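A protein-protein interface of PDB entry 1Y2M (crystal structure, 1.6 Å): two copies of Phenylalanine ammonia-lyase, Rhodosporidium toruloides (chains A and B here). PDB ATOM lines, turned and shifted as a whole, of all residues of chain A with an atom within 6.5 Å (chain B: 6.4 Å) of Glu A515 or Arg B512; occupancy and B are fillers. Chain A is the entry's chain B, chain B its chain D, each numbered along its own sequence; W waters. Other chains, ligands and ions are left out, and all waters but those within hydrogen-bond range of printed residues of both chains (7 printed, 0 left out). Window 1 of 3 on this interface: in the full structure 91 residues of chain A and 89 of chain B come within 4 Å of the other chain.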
ATOM      1  N   LEU A 429     -24.407 -30.263   6.539  1.00  0.00           N
ATOM      2  CA  LEU A 429     -25.234 -29.265   5.820  1.00  0.00           C
ATOM      3  C   LEU A 429     -26.425 -29.972   5.163  1.00  0.00           C
ATOM      4  O   LEU A 429     -27.559 -29.454   5.138  1.00  0.00           O
ATOM      5  CB  LEU A 429     -24.407 -28.470   4.816  1.00  0.00           C
ATOM      6  CG  LEU A 429     -23.345 -27.573   5.451  1.00  0.00           C
ATOM      7  CD1 LEU A 429     -22.367 -27.080   4.404  1.00  0.00           C
ATOM      8  CD2 LEU A 429     -24.003 -26.422   6.246  1.00  0.00           C
ATOM      9  N   GLU A 480     -30.312 -31.247  -4.117  1.00  0.00           N
ATOM     10  CA  GLU A 480     -28.967 -30.789  -4.499  1.00  0.00           C
ATOM     11  C   GLU A 480     -27.949 -30.950  -3.364  1.00  0.00           C
ATOM     12  O   GLU A 480     -26.841 -31.452  -3.592  1.00  0.00           O
ATOM     13  CB  GLU A 480     -29.004 -29.360  -5.018  1.00  0.00           C
ATOM     14  CG  GLU A 480     -27.659 -28.939  -5.539  1.00  0.00           C
ATOM     15  CD  GLU A 480     -27.707 -27.651  -6.372  1.00  0.00           C
ATOM     16  OE1 GLU A 480     -28.833 -27.258  -6.828  1.00  0.00           O
ATOM     17  OE2 GLU A 480     -26.621 -27.006  -6.551  1.00  0.00           O
ATOM     18  N   LEU A 481     -28.381 -30.627  -2.140  1.00  0.00           N
ATOM     19  CA  LEU A 481     -27.543 -30.899  -0.974  1.00  0.00           C
ATOM     20  C   LEU A 481     -27.162 -32.359  -0.828  1.00  0.00           C
ATOM     21  O   LEU A 481     -26.031 -32.682  -0.430  1.00  0.00           O
ATOM     22  CB  LEU A 481     -28.210 -30.410   0.305  1.00  0.00           C
ATOM     23  CG  LEU A 481     -28.245 -28.893   0.459  1.00  0.00           C
ATOM     24  CD1 LEU A 481     -29.285 -28.466   1.563  1.00  0.00           C
ATOM     25  CD2 LEU A 481     -26.860 -28.328   0.757  1.00  0.00           C
ATOM     26  N   HIS A 483     -26.745 -34.801  -3.125  1.00  0.00           N
ATOM     27  CA  HIS A 483     -25.666 -35.195  -4.039  1.00  0.00           C
ATOM     28  C   HIS A 483     -24.353 -34.539  -3.660  1.00  0.00           C
ATOM     29  O   HIS A 483     -23.296 -35.157  -3.746  1.00  0.00           O
ATOM     30  CB  HIS A 483     -26.088 -34.854  -5.467  1.00  0.00           C
ATOM     31  CG  HIS A 483     -25.005 -34.966  -6.465  1.00  0.00           C
ATOM     32  ND1 HIS A 483     -24.175 -33.920  -6.796  1.00  0.00           N
ATOM     33  CD2 HIS A 483     -24.641 -36.012  -7.245  1.00  0.00           C
ATOM     34  CE1 HIS A 483     -23.327 -34.326  -7.728  1.00  0.00           C
ATOM     35  NE2 HIS A 483     -23.616 -35.582  -8.043  1.00  0.00           N
ATOM     36  N   LEU A 484     -24.397 -33.275  -3.252  1.00  0.00           N
ATOM     37  CA  LEU A 484     -23.161 -32.568  -2.863  1.00  0.00           C
ATOM     38  C   LEU A 484     -22.440 -33.338  -1.759  1.00  0.00           C
ATOM     39  O   LEU A 484     -21.206 -33.307  -1.705  1.00  0.00           O
ATOM     40  CB  LEU A 484     -23.468 -31.135  -2.404  1.00  0.00           C
ATOM     41  CG  LEU A 484     -23.527 -30.157  -3.576  1.00  0.00           C
ATOM     42  CD1 LEU A 484     -24.231 -28.850  -3.201  1.00  0.00           C
ATOM     43  CD2 LEU A 484     -22.088 -29.845  -4.067  1.00  0.00           C
ATOM     44  N   ALA A 510     -13.418 -28.394   0.111  1.00  0.00           N
ATOM     45  CA  ALA A 510     -13.825 -27.074   0.627  1.00  0.00           C
ATOM     46  C   ALA A 510     -14.771 -26.349  -0.336  1.00  0.00           C
ATOM     47  O   ALA A 510     -15.755 -25.676   0.052  1.00  0.00           O
ATOM     48  CB  ALA A 510     -12.638 -26.270   0.980  1.00  0.00           C
ATOM     49  N   ARG A 511     -14.454 -26.475  -1.630  1.00  0.00           N
ATOM     50  CA  ARG A 511     -15.282 -25.895  -2.683  1.00  0.00           C
ATOM     51  C   ARG A 511     -16.663 -26.477  -2.652  1.00  0.00           C
ATOM     52  O   ARG A 511     -17.666 -25.724  -2.749  1.00  0.00           O
ATOM     53  CB  ARG A 511     -14.641 -26.066  -4.051  1.00  0.00           C
ATOM     54  CG  ARG A 511     -13.479 -25.090  -4.337  1.00  0.00           C
ATOM     55  CD  ARG A 511     -12.739 -25.337  -5.621  1.00  0.00           C
ATOM     56  NE  ARG A 511     -13.712 -25.607  -6.654  1.00  0.00           N
ATOM     57  CZ  ARG A 511     -13.709 -26.633  -7.496  1.00  0.00           C
ATOM     58  NH1 ARG A 511     -12.733 -27.550  -7.513  1.00  0.00           N
ATOM     59  NH2 ARG A 511     -14.757 -26.753  -8.286  1.00  0.00           N
ATOM     60  N   ARG A 512     -16.740 -27.800  -2.524  1.00  0.00           N
ATOM     61  CA  ARG A 512     -18.073 -28.415  -2.513  1.00  0.00           C
ATOM     62  C   ARG A 512     -18.837 -28.030  -1.259  1.00  0.00           C
ATOM     63  O   ARG A 512     -20.050 -27.735  -1.319  1.00  0.00           O
ATOM     64  CB  ARG A 512     -17.966 -29.940  -2.689  1.00  0.00           C
ATOM     65  CG  ARG A 512     -17.388 -30.405  -3.996  1.00  0.00           C
ATOM     66  CD  ARG A 512     -18.142 -29.801  -5.174  1.00  0.00           C
ATOM     67  NE  ARG A 512     -17.665 -30.335  -6.438  1.00  0.00           N
ATOM     68  CZ  ARG A 512     -17.620 -29.705  -7.583  1.00  0.00           C
ATOM     69  NH1 ARG A 512     -17.798 -28.366  -7.668  1.00  0.00           N
ATOM     70  NH2 ARG A 512     -17.209 -30.406  -8.649  1.00  0.00           N
ATOM     71  N   THR A 513     -18.160 -27.958  -0.116  1.00  0.00           N
ATOM     72  CA  THR A 513     -18.865 -27.564   1.119  1.00  0.00           C
ATOM     73  C   THR A 513     -19.330 -26.087   1.022  1.00  0.00           C
ATOM     74  O   THR A 513     -20.373 -25.761   1.551  1.00  0.00           O
ATOM     75  CB  THR A 513     -17.940 -27.787   2.323  1.00  0.00           C
ATOM     76  OG1 THR A 513     -17.538 -29.162   2.302  1.00  0.00           O
ATOM     77  CG2 THR A 513     -18.638 -27.383   3.628  1.00  0.00           C
ATOM     78  N   THR A 514     -18.553 -25.190   0.360  1.00  0.00           N
ATOM     79  CA  THR A 514     -18.939 -23.809   0.153  1.00  0.00           C
ATOM     80  C   THR A 514     -20.196 -23.762  -0.683  1.00  0.00           C
ATOM     81  O   THR A 514     -21.091 -22.951  -0.401  1.00  0.00           O
ATOM     82  CB  THR A 514     -17.780 -23.055  -0.512  1.00  0.00           C
ATOM     83  OG1 THR A 514     -16.628 -23.058   0.360  1.00  0.00           O
ATOM     84  CG2 THR A 514     -18.180 -21.658  -0.814  1.00  0.00           C
ATOM     85  N   GLU A 515     -20.312 -24.647  -1.691  1.00  0.00           N
ATOM     86  CA  GLU A 515     -21.519 -24.687  -2.514  1.00  0.00           C
ATOM     87  C   GLU A 515     -22.690 -25.192  -1.661  1.00  0.00           C
ATOM     88  O   GLU A 515     -23.811 -24.661  -1.767  1.00  0.00           O
ATOM     89  CB  GLU A 515     -21.324 -25.570  -3.730  1.00  0.00           C
ATOM     90  CG  GLU A 515     -22.528 -25.466  -4.677  1.00  0.00           C
ATOM     91  CD  GLU A 515     -22.385 -26.138  -6.035  1.00  0.00           C
ATOM     92  OE1 GLU A 515     -21.284 -26.665  -6.394  1.00  0.00           O
ATOM     93  OE2 GLU A 515     -23.410 -26.138  -6.778  1.00  0.00           O
ATOM     94  N   SER A 516     -22.460 -26.193  -0.801  1.00  0.00           N
ATOM     95  CA  SER A 516     -23.534 -26.640   0.079  1.00  0.00           C
ATOM     96  C   SER A 516     -23.980 -25.523   1.023  1.00  0.00           C
ATOM     97  O   SER A 516     -25.179 -25.355   1.269  1.00  0.00           O
ATOM     98  CB  SER A 516     -23.138 -27.852   0.900  1.00  0.00           C
ATOM     99  OG  SER A 516     -22.986 -28.964   0.032  1.00  0.00           O
ATOM    100  N   ASN A 517     -23.050 -24.686   1.499  1.00  0.00           N
ATOM    101  CA  ASN A 517     -23.453 -23.518   2.288  1.00  0.00           C
ATOM    102  C   ASN A 517     -24.405 -22.649   1.510  1.00  0.00           C
ATOM    103  O   ASN A 517     -25.407 -22.168   2.054  1.00  0.00           O
ATOM    104  CB  ASN A 517     -22.305 -22.633   2.807  1.00  0.00           C
ATOM    105  CG  ASN A 517     -21.571 -23.217   3.978  1.00  0.00           C
ATOM    106  OD1 ASN A 517     -22.155 -23.920   4.793  1.00  0.00           O
ATOM    107  ND2 ASN A 517     -20.282 -22.834   4.130  1.00  0.00           N
ATOM    108  N   ASP A 518     -24.125 -22.451   0.230  1.00  0.00           N
ATOM    109  CA  ASP A 518     -24.897 -21.568  -0.618  1.00  0.00           C
ATOM    110  C   ASP A 518     -26.300 -22.136  -0.801  1.00  0.00           C
ATOM    111  O   ASP A 518     -27.331 -21.451  -0.633  1.00  0.00           O
ATOM    112  CB  ASP A 518     -24.207 -21.446  -1.973  1.00  0.00           C
ATOM    113  CG  ASP A 518     -24.734 -20.270  -2.811  1.00  0.00           C
ATOM    114  OD1 ASP A 518     -25.199 -19.221  -2.243  1.00  0.00           O
ATOM    115  OD2 ASP A 518     -24.621 -20.379  -4.055  1.00  0.00           O
ATOM    116  N   VAL A 519     -26.361 -23.425  -1.152  1.00  0.00           N
ATOM    117  CA  VAL A 519     -27.669 -24.079  -1.333  1.00  0.00           C
ATOM    118  C   VAL A 519     -28.466 -24.104  -0.071  1.00  0.00           C
ATOM    119  O   VAL A 519     -29.704 -23.877  -0.102  1.00  0.00           O
ATOM    120  CB  VAL A 519     -27.490 -25.451  -1.941  1.00  0.00           C
ATOM    121  CG1 VAL A 519     -28.815 -26.184  -2.094  1.00  0.00           C
ATOM    122  CG2 VAL A 519     -26.781 -25.287  -3.279  1.00  0.00           C
ATOM    123  N   LEU A 520     -27.809 -24.397   1.055  1.00  0.00           N
ATOM    124  CA  LEU A 520     -28.533 -24.395   2.340  1.00  0.00           C
ATOM    125  C   LEU A 520     -29.036 -22.983   2.617  1.00  0.00           C
ATOM    126  O   LEU A 520     -30.116 -22.834   3.193  1.00  0.00           O
ATOM    127  CB  LEU A 520     -27.666 -24.886   3.499  1.00  0.00           C
ATOM    128  CG  LEU A 520     -28.384 -25.047   4.851  1.00  0.00           C
ATOM    129  CD1 LEU A 520     -29.702 -25.808   4.783  1.00  0.00           C
ATOM    130  CD2 LEU A 520     -27.520 -25.752   5.899  1.00  0.00           C
ATOM    131  N   ARG B 206     -31.600 -22.165  -9.743  1.00  0.00           N
ATOM    132  CA  ARG B 206     -32.158 -23.196  -8.901  1.00  0.00           C
ATOM    133  C   ARG B 206     -33.611 -22.970  -8.499  1.00  0.00           C
ATOM    134  O   ARG B 206     -34.116 -21.843  -8.491  1.00  0.00           O
ATOM    135  CB  ARG B 206     -31.314 -23.320  -7.612  1.00  0.00           C
ATOM    136  CG  ARG B 206     -29.839 -23.665  -7.847  1.00  0.00           C
ATOM    137  CD  ARG B 206     -29.105 -23.914  -6.493  1.00  0.00           C
ATOM    138  NE  ARG B 206     -27.714 -24.369  -6.604  1.00  0.00           N
ATOM    139  CZ  ARG B 206     -26.657 -23.598  -6.465  1.00  0.00           C
ATOM    140  NH1 ARG B 206     -26.781 -22.271  -6.324  1.00  0.00           N
ATOM    141  NH2 ARG B 206     -25.452 -24.156  -6.456  1.00  0.00           N
ATOM    142  N   ARG B 426     -22.787 -38.103 -17.362  1.00  0.00           N
ATOM    143  CA  ARG B 426     -21.840 -37.634 -16.353  1.00  0.00           C
ATOM    144  C   ARG B 426     -20.935 -38.735 -15.859  1.00  0.00           C
ATOM    145  O   ARG B 426     -19.763 -38.504 -15.619  1.00  0.00           O
ATOM    146  CB  ARG B 426     -22.599 -36.943 -15.209  1.00  0.00           C
ATOM    147  CG  ARG B 426     -21.705 -36.197 -14.273  1.00  0.00           C
ATOM    148  CD  ARG B 426     -22.495 -35.231 -13.360  1.00  0.00           C
ATOM    149  NE  ARG B 426     -23.382 -35.974 -12.463  1.00  0.00           N
ATOM    150  CZ  ARG B 426     -24.705 -36.175 -12.602  1.00  0.00           C
ATOM    151  NH1 ARG B 426     -25.389 -35.741 -13.650  1.00  0.00           N
ATOM    152  NH2 ARG B 426     -25.376 -36.810 -11.663  1.00  0.00           N
ATOM    153  N   LEU B 429     -18.394 -39.153 -18.634  1.00  0.00           N
ATOM    154  CA  LEU B 429     -17.335 -38.132 -18.671  1.00  0.00           C
ATOM    155  C   LEU B 429     -16.245 -38.488 -17.629  1.00  0.00           C
ATOM    156  O   LEU B 429     -15.049 -38.282 -17.846  1.00  0.00           O
ATOM    157  CB  LEU B 429     -17.919 -36.761 -18.401  1.00  0.00           C
ATOM    158  CG  LEU B 429     -18.946 -36.300 -19.453  1.00  0.00           C
ATOM    159  CD1 LEU B 429     -19.767 -35.119 -18.929  1.00  0.00           C
ATOM    160  CD2 LEU B 429     -18.148 -35.927 -20.738  1.00  0.00           C
ATOM    161  N   LEU B 484     -18.301 -35.759  -9.036  1.00  0.00           N
ATOM    162  CA  LEU B 484     -19.449 -35.213  -9.809  1.00  0.00           C
ATOM    163  C   LEU B 484     -20.357 -36.356 -10.318  1.00  0.00           C
ATOM    164  O   LEU B 484     -21.582 -36.159 -10.440  1.00  0.00           O
ATOM    165  CB  LEU B 484     -18.992 -34.400 -11.006  1.00  0.00           C
ATOM    166  CG  LEU B 484     -18.670 -32.953 -10.676  1.00  0.00           C
ATOM    167  CD1 LEU B 484     -17.715 -32.376 -11.674  1.00  0.00           C
ATOM    168  CD2 LEU B 484     -19.974 -32.158 -10.611  1.00  0.00           C
ATOM    169  N   ASN B 486     -21.537 -39.162  -9.182  1.00  0.00           N
ATOM    170  CA  ASN B 486     -22.606 -39.794  -8.369  1.00  0.00           C
ATOM    171  C   ASN B 486     -23.938 -39.279  -8.879  1.00  0.00           C
ATOM    172  O   ASN B 486     -24.014 -38.188  -9.410  1.00  0.00           O
ATOM    173  CB  ASN B 486     -22.442 -39.463  -6.875  1.00  0.00           C
ATOM    174  CG  ASN B 486     -21.167 -40.082  -6.298  1.00  0.00           C
ATOM    175  OD1 ASN B 486     -20.939 -41.252  -6.538  1.00  0.00           O
ATOM    176  ND2 ASN B 486     -20.349 -39.306  -5.598  1.00  0.00           N
ATOM    177  N   VAL B 488     -27.651 -37.758  -9.205  1.00  0.00           N
ATOM    178  CA  VAL B 488     -28.537 -36.771  -8.579  1.00  0.00           C
ATOM    179  C   VAL B 488     -29.929 -37.418  -8.317  1.00  0.00           C
ATOM    180  O   VAL B 488     -30.638 -37.108  -7.359  1.00  0.00           O
ATOM    181  CB  VAL B 488     -28.664 -35.491  -9.484  1.00  0.00           C
ATOM    182  CG1 VAL B 488     -29.902 -34.657  -9.175  1.00  0.00           C
ATOM    183  CG2 VAL B 488     -27.365 -34.707  -9.419  1.00  0.00           C
ATOM    184  N   LEU B 507     -32.933 -30.922 -14.414  1.00  0.00           N
ATOM    185  CA  LEU B 507     -32.110 -29.708 -14.572  1.00  0.00           C
ATOM    186  C   LEU B 507     -30.895 -29.737 -13.655  1.00  0.00           C
ATOM    187  O   LEU B 507     -29.790 -29.345 -14.064  1.00  0.00           O
ATOM    188  CB  LEU B 507     -32.913 -28.436 -14.341  1.00  0.00           C
ATOM    189  CG  LEU B 507     -32.107 -27.177 -14.687  1.00  0.00           C
ATOM    190  CD1 LEU B 507     -31.684 -27.084 -16.152  1.00  0.00           C
ATOM    191  CD2 LEU B 507     -32.979 -25.991 -14.321  1.00  0.00           C
ATOM    192  N   ILE B 508     -31.089 -30.190 -12.407  1.00  0.00           N
ATOM    193  CA  ILE B 508     -29.950 -30.313 -11.486  1.00  0.00           C
ATOM    194  C   ILE B 508     -28.925 -31.292 -12.071  1.00  0.00           C
ATOM    195  O   ILE B 508     -27.704 -31.003 -12.110  1.00  0.00           O
ATOM    196  CB  ILE B 508     -30.356 -30.709 -10.068  1.00  0.00           C
ATOM    197  CG1 ILE B 508     -31.360 -29.718  -9.489  1.00  0.00           C
ATOM    198  CG2 ILE B 508     -29.126 -30.904  -9.180  1.00  0.00           C
ATOM    199  CD1 ILE B 508     -32.089 -30.218  -8.301  1.00  0.00           C
ATOM    200  N   SER B 509     -29.385 -32.409 -12.582  1.00  0.00           N
ATOM    201  CA  SER B 509     -28.481 -33.360 -13.204  1.00  0.00           C
ATOM    202  C   SER B 509     -27.720 -32.734 -14.383  1.00  0.00           C
ATOM    203  O   SER B 509     -26.496 -32.915 -14.554  1.00  0.00           O
ATOM    204  CB  SER B 509     -29.215 -34.598 -13.665  1.00  0.00           C
ATOM    205  OG  SER B 509     -28.336 -35.634 -14.048  1.00  0.00           O
ATOM    206  N   ALA B 510     -28.473 -32.060 -15.240  1.00  0.00           N
ATOM    207  CA  ALA B 510     -27.890 -31.358 -16.367  1.00  0.00           C
ATOM    208  C   ALA B 510     -26.818 -30.343 -15.999  1.00  0.00           C
ATOM    209  O   ALA B 510     -25.783 -30.231 -16.654  1.00  0.00           O
ATOM    210  CB  ALA B 510     -28.951 -30.709 -17.206  1.00  0.00           C
ATOM    211  N   ARG B 511     -27.083 -29.585 -14.936  1.00  0.00           N
ATOM    212  CA  ARG B 511     -26.062 -28.653 -14.408  1.00  0.00           C
ATOM    213  C   ARG B 511     -24.805 -29.393 -13.989  1.00  0.00           C
ATOM    214  O   ARG B 511     -23.713 -28.971 -14.303  1.00  0.00           O
ATOM    215  CB  ARG B 511     -26.605 -27.859 -13.235  1.00  0.00           C
ATOM    216  CG  ARG B 511     -27.590 -26.779 -13.639  1.00  0.00           C
ATOM    217  CD  ARG B 511     -28.301 -26.189 -12.450  1.00  0.00           C
ATOM    218  NE  ARG B 511     -27.333 -25.886 -11.407  1.00  0.00           N
ATOM    219  CZ  ARG B 511     -27.456 -26.220 -10.130  1.00  0.00           C
ATOM    220  NH1 ARG B 511     -28.572 -26.756  -9.653  1.00  0.00           N
ATOM    221  NH2 ARG B 511     -26.426 -25.968  -9.340  1.00  0.00           N
ATOM    222  N   ARG B 512     -24.951 -30.528 -13.317  1.00  0.00           N
ATOM    223  CA  ARG B 512     -23.782 -31.279 -12.901  1.00  0.00           C
ATOM    224  C   ARG B 512     -23.009 -31.786 -14.089  1.00  0.00           C
ATOM    225  O   ARG B 512     -21.741 -31.744 -14.108  1.00  0.00           O
ATOM    226  CB  ARG B 512     -24.145 -32.377 -11.911  1.00  0.00           C
ATOM    227  CG  ARG B 512     -24.702 -31.880 -10.567  1.00  0.00           C
ATOM    228  CD  ARG B 512     -23.794 -30.823  -9.919  1.00  0.00           C
ATOM    229  NE  ARG B 512     -24.244 -30.472  -8.559  1.00  0.00           N
ATOM    230  CZ  ARG B 512     -24.208 -29.236  -8.044  1.00  0.00           C
ATOM    231  NH1 ARG B 512     -23.759 -28.192  -8.716  1.00  0.00           N
ATOM    232  NH2 ARG B 512     -24.591 -29.061  -6.778  1.00  0.00           N
ATOM    233  N   THR B 513     -23.732 -32.264 -15.119  1.00  0.00           N
ATOM    234  CA  THR B 513     -23.060 -32.816 -16.282  1.00  0.00           C
ATOM    235  C   THR B 513     -22.332 -31.694 -17.040  1.00  0.00           C
ATOM    236  O   THR B 513     -21.252 -31.912 -17.596  1.00  0.00           O
ATOM    237  CB  THR B 513     -24.068 -33.523 -17.145  1.00  0.00           C
ATOM    238  OG1 THR B 513     -24.688 -34.552 -16.343  1.00  0.00           O
ATOM    239  CG2 THR B 513     -23.407 -34.110 -18.376  1.00  0.00           C
ATOM    240  N   THR B 514     -22.936 -30.530 -17.039  1.00  0.00           N
ATOM    241  CA  THR B 514     -22.316 -29.365 -17.660  1.00  0.00           C
ATOM    242  C   THR B 514     -20.980 -29.036 -16.957  1.00  0.00           C
ATOM    243  O   THR B 514     -19.969 -28.714 -17.608  1.00  0.00           O
ATOM    244  CB  THR B 514     -23.255 -28.174 -17.684  1.00  0.00           C
ATOM    245  OG1 THR B 514     -24.443 -28.537 -18.397  1.00  0.00           O
ATOM    246  CG2 THR B 514     -22.584 -26.991 -18.297  1.00  0.00           C
ATOM    247  N   GLU B 515     -20.978 -29.090 -15.629  1.00  0.00           N
ATOM    248  CA  GLU B 515     -19.735 -28.901 -14.864  1.00  0.00           C
ATOM    249  C   GLU B 515     -18.689 -30.006 -15.172  1.00  0.00           C
ATOM    250  O   GLU B 515     -17.488 -29.735 -15.351  1.00  0.00           O
ATOM    251  CB  GLU B 515     -20.013 -28.843 -13.375  1.00  0.00           C
ATOM    252  CG  GLU B 515     -18.747 -28.597 -12.560  1.00  0.00           C
ATOM    253  CD  GLU B 515     -18.973 -28.141 -11.093  1.00  0.00           C
ATOM    254  OE1 GLU B 515     -20.137 -28.075 -10.624  1.00  0.00           O
ATOM    255  OE2 GLU B 515     -17.942 -27.844 -10.405  1.00  0.00           O
ATOM    256  N   SER B 516     -19.136 -31.263 -15.293  1.00  0.00           N
ATOM    257  CA  SER B 516     -18.238 -32.331 -15.731  1.00  0.00           C
ATOM    258  C   SER B 516     -17.656 -32.085 -17.110  1.00  0.00           C
ATOM    259  O   SER B 516     -16.446 -32.301 -17.342  1.00  0.00           O
ATOM    260  CB  SER B 516     -18.943 -33.681 -15.643  1.00  0.00           C
ATOM    261  OG  SER B 516     -19.211 -34.056 -14.291  1.00  0.00           O
ATOM    262  N   ASN B 517     -18.448 -31.549 -18.037  1.00  0.00           N
ATOM    263  CA  ASN B 517     -17.892 -31.201 -19.346  1.00  0.00           C
ATOM    264  C   ASN B 517     -16.749 -30.193 -19.155  1.00  0.00           C
ATOM    265  O   ASN B 517     -15.723 -30.243 -19.815  1.00  0.00           O
ATOM    266  CB  ASN B 517     -18.959 -30.588 -20.290  1.00  0.00           C
ATOM    267  CG  ASN B 517     -19.815 -31.655 -20.991  1.00  0.00           C
ATOM    268  OD1 ASN B 517     -19.360 -32.795 -21.213  1.00  0.00           O
ATOM    269  ND2 ASN B 517     -21.060 -31.266 -21.358  1.00  0.00           N
HETATM  270  O   HOH W   1     -23.711 -25.118  -9.841  1.00  0.00           O
HETATM  271  O   HOH W   2     -17.334 -25.382  -8.715  1.00  0.00           O
HETATM  272  O   HOH W   3     -20.575 -25.993  -8.994  1.00  0.00           O
HETATM  273  O   HOH W   4     -25.720 -31.608  -6.150  1.00  0.00           O
HETATM  274  O   HOH W   5     -20.878 -29.164  -7.896  1.00  0.00           O
HETATM  275  O   HOH W   6     -21.571 -36.489  -5.472  1.00  0.00           O
HETATM  276  O   HOH W   7     -23.501 -22.056  -5.787  1.00  0.00           O
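Leu A484 touches Arg B512, and with the chains exchanged Arg A512 touches Leu B484.
Arg A511 touches Glu B515, and with the chains exchanged Glu A515 touches Arg B511.
Arg A512 touches Glu B515, and with the chains exchanged Glu A515 touches Arg B512.
10 positions are printed for both chains.
Of the 16 pairs that touch across the chains among the printed residues, 6 have their exchanged pair printed and touching as well.
Among the printed residues, merely in contact across the chains: His A483 with Val B488, His A483 with Arg B512, Leu A484 with Arg B512, Arg A512 with Leu B484 and Val A519 with Arg B206.
Water W7 lies within hydrogen-bond range of the side-chain carboxylate (OD2) of Asp A518 (2.7 Å) and the guanidinium group (NH2) of Arg B206 (2.9 Å).
Water W3 lies within hydrogen-bond range of the side-chain carboxylate (OE1) of Glu B515 and the side-chain carboxylate (OE1) of Glu A515.
Water W6 bridges O of His A483 (2.8 Å) and ND2 of Asn B486 (3.1 Å).
Water W4 lies within hydrogen-bond range of O of Glu A480 (2.8 Å), ND1 of His A483 (2.9 Å) and NH2 of Arg B512 (2.9 Å).
Water W1 lies within hydrogen-bond range of NH2 of Arg B511, OE2 of Glu A515 and NH1 of Arg B512.
Water W2 lies within hydrogen-bond range of the guanidinium group of Arg A511 (3.0 Å), the side-chain carboxylate of Glu B515 (3.0 Å) and the guanidinium group of Arg A512 (3.2 Å).
Printed residues of chain A that touch a printed residue of chain B: Glu A480, His A483, Leu A484, Arg A511, Arg A512, Glu A515, Asp A518 and Val A519.
Hydrophobic or aromatic side chains of chain A within 4 Å of the printed part of chain B: His A483, Leu A484 and Val A519.
Along chain A the printed residues that touch a printed residue of chain B span positions 480 to 519.
Among the printed residues, 16 pairs touch across the chains.
Among the printed residues, Asp or Glu carboxylates within 4 Å of a Lys or Arg side-chain nitrogen of the other chain: Glu A480 with Arg B206 (2.9 Å), Glu A480 with Arg B511 (2.9 Å), Glu A480 with Arg B512 (2.9 Å), Arg A511 with Glu B515 (3.98 Å), Arg A512 with Glu B515 (2.8 Å), Glu A515 with Arg B206 (2.9 Å), Glu A515 with Arg B511 (3.96 Å), Glu A515 with Arg B512 (2.8 Å) and Asp A518 with Arg B206 (3.7 Å).
The backbone carbonyl oxygen (O) of Leu B484 lies within hydrogen-bond range of a ring nitrogen (NE2) of His A483 (3.2 Å).
OE2 of Glu A515 lies within salt-bridge range of NH2 of Arg B206 (2.9 Å).
The side-chain carboxylate (OE2) of Glu A515 lies within salt-bridge range of the guanidinium group (NH2) of Arg B511.
OE2 of Glu B515 is in salt-bridge range of NH2 of Arg A511, at 3.98 Å.
The side-chain carboxylate of Glu A480 lies within salt-bridge range of the guanidinium group of Arg B206, at 2.9 Å.
The guanidinium group (NH1) of Arg B206 is in salt-bridge range of the side-chain carboxylate (OD2) of Asp A518, at 3.7 Å.
The side-chain carboxylate (OE2) of Glu A480 lies within salt-bridge range of the guanidinium group (NH2) of Arg B512, at 2.9 Å.
The side-chain carboxylate (OE1) of Glu A480 is in salt-bridge range of the guanidinium group (NH1) of Arg B511 (2.9 Å).
The guanidinium group (NH1) of Arg A512 lies within salt-bridge range of the side-chain carboxylate (OE2) of Glu B515, at 2.8 Å.
A ring nitrogen (NE2) of His A483 is in hydrogen-bond range of the backbone carbonyl oxygen (O) of Asn B486, 3.0 Å away.
OE2 of Glu A515 is in salt-bridge range of NH1 of Arg B512 (2.8 Å).
Of chain B, only Arg B206 (2.9 Å), Arg B511 (3.96 Å) and Arg B512 (2.8 Å) come within 4 Å of Glu A515.
Printed residues of chain A within 4 Å of Arg B512: Glu A480, His A483, Leu A484 and Glu A515.
Printed residues of chain B within 4 Å of Glu A480: Arg B206, Arg B511 and Arg B512.
Of the printed residues of chain B, His A483 touches Leu B484 (3.2 Å), Asn B486 (3.0 Å), Val B488 (3.7 Å) and Arg B512 (3.9 Å).
Of the printed residues of chain A, Arg B206 touches Glu A480 (2.9 Å), Glu A515 (2.9 Å), Asp A518 (3.7 Å) and Val A519 (3.6 Å).
The backbone carbonyl oxygen of Arg B512 lies within hydrogen-bond range of the side-chain hydroxyl of Ser B516 (3.4 Å).
The backbone carbonyl oxygen (O) of Leu B484 lies within hydrogen-bond range of the guanidinium group (NE) of Arg B426.
NH2 of Arg B426 is in hydrogen-bond range of O of Asn B486, 3.0 Å away.
The side-chain hydroxyl (OG) of Ser A516 lies within hydrogen-bond range of the backbone carbonyl oxygen (O) of Arg A512.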
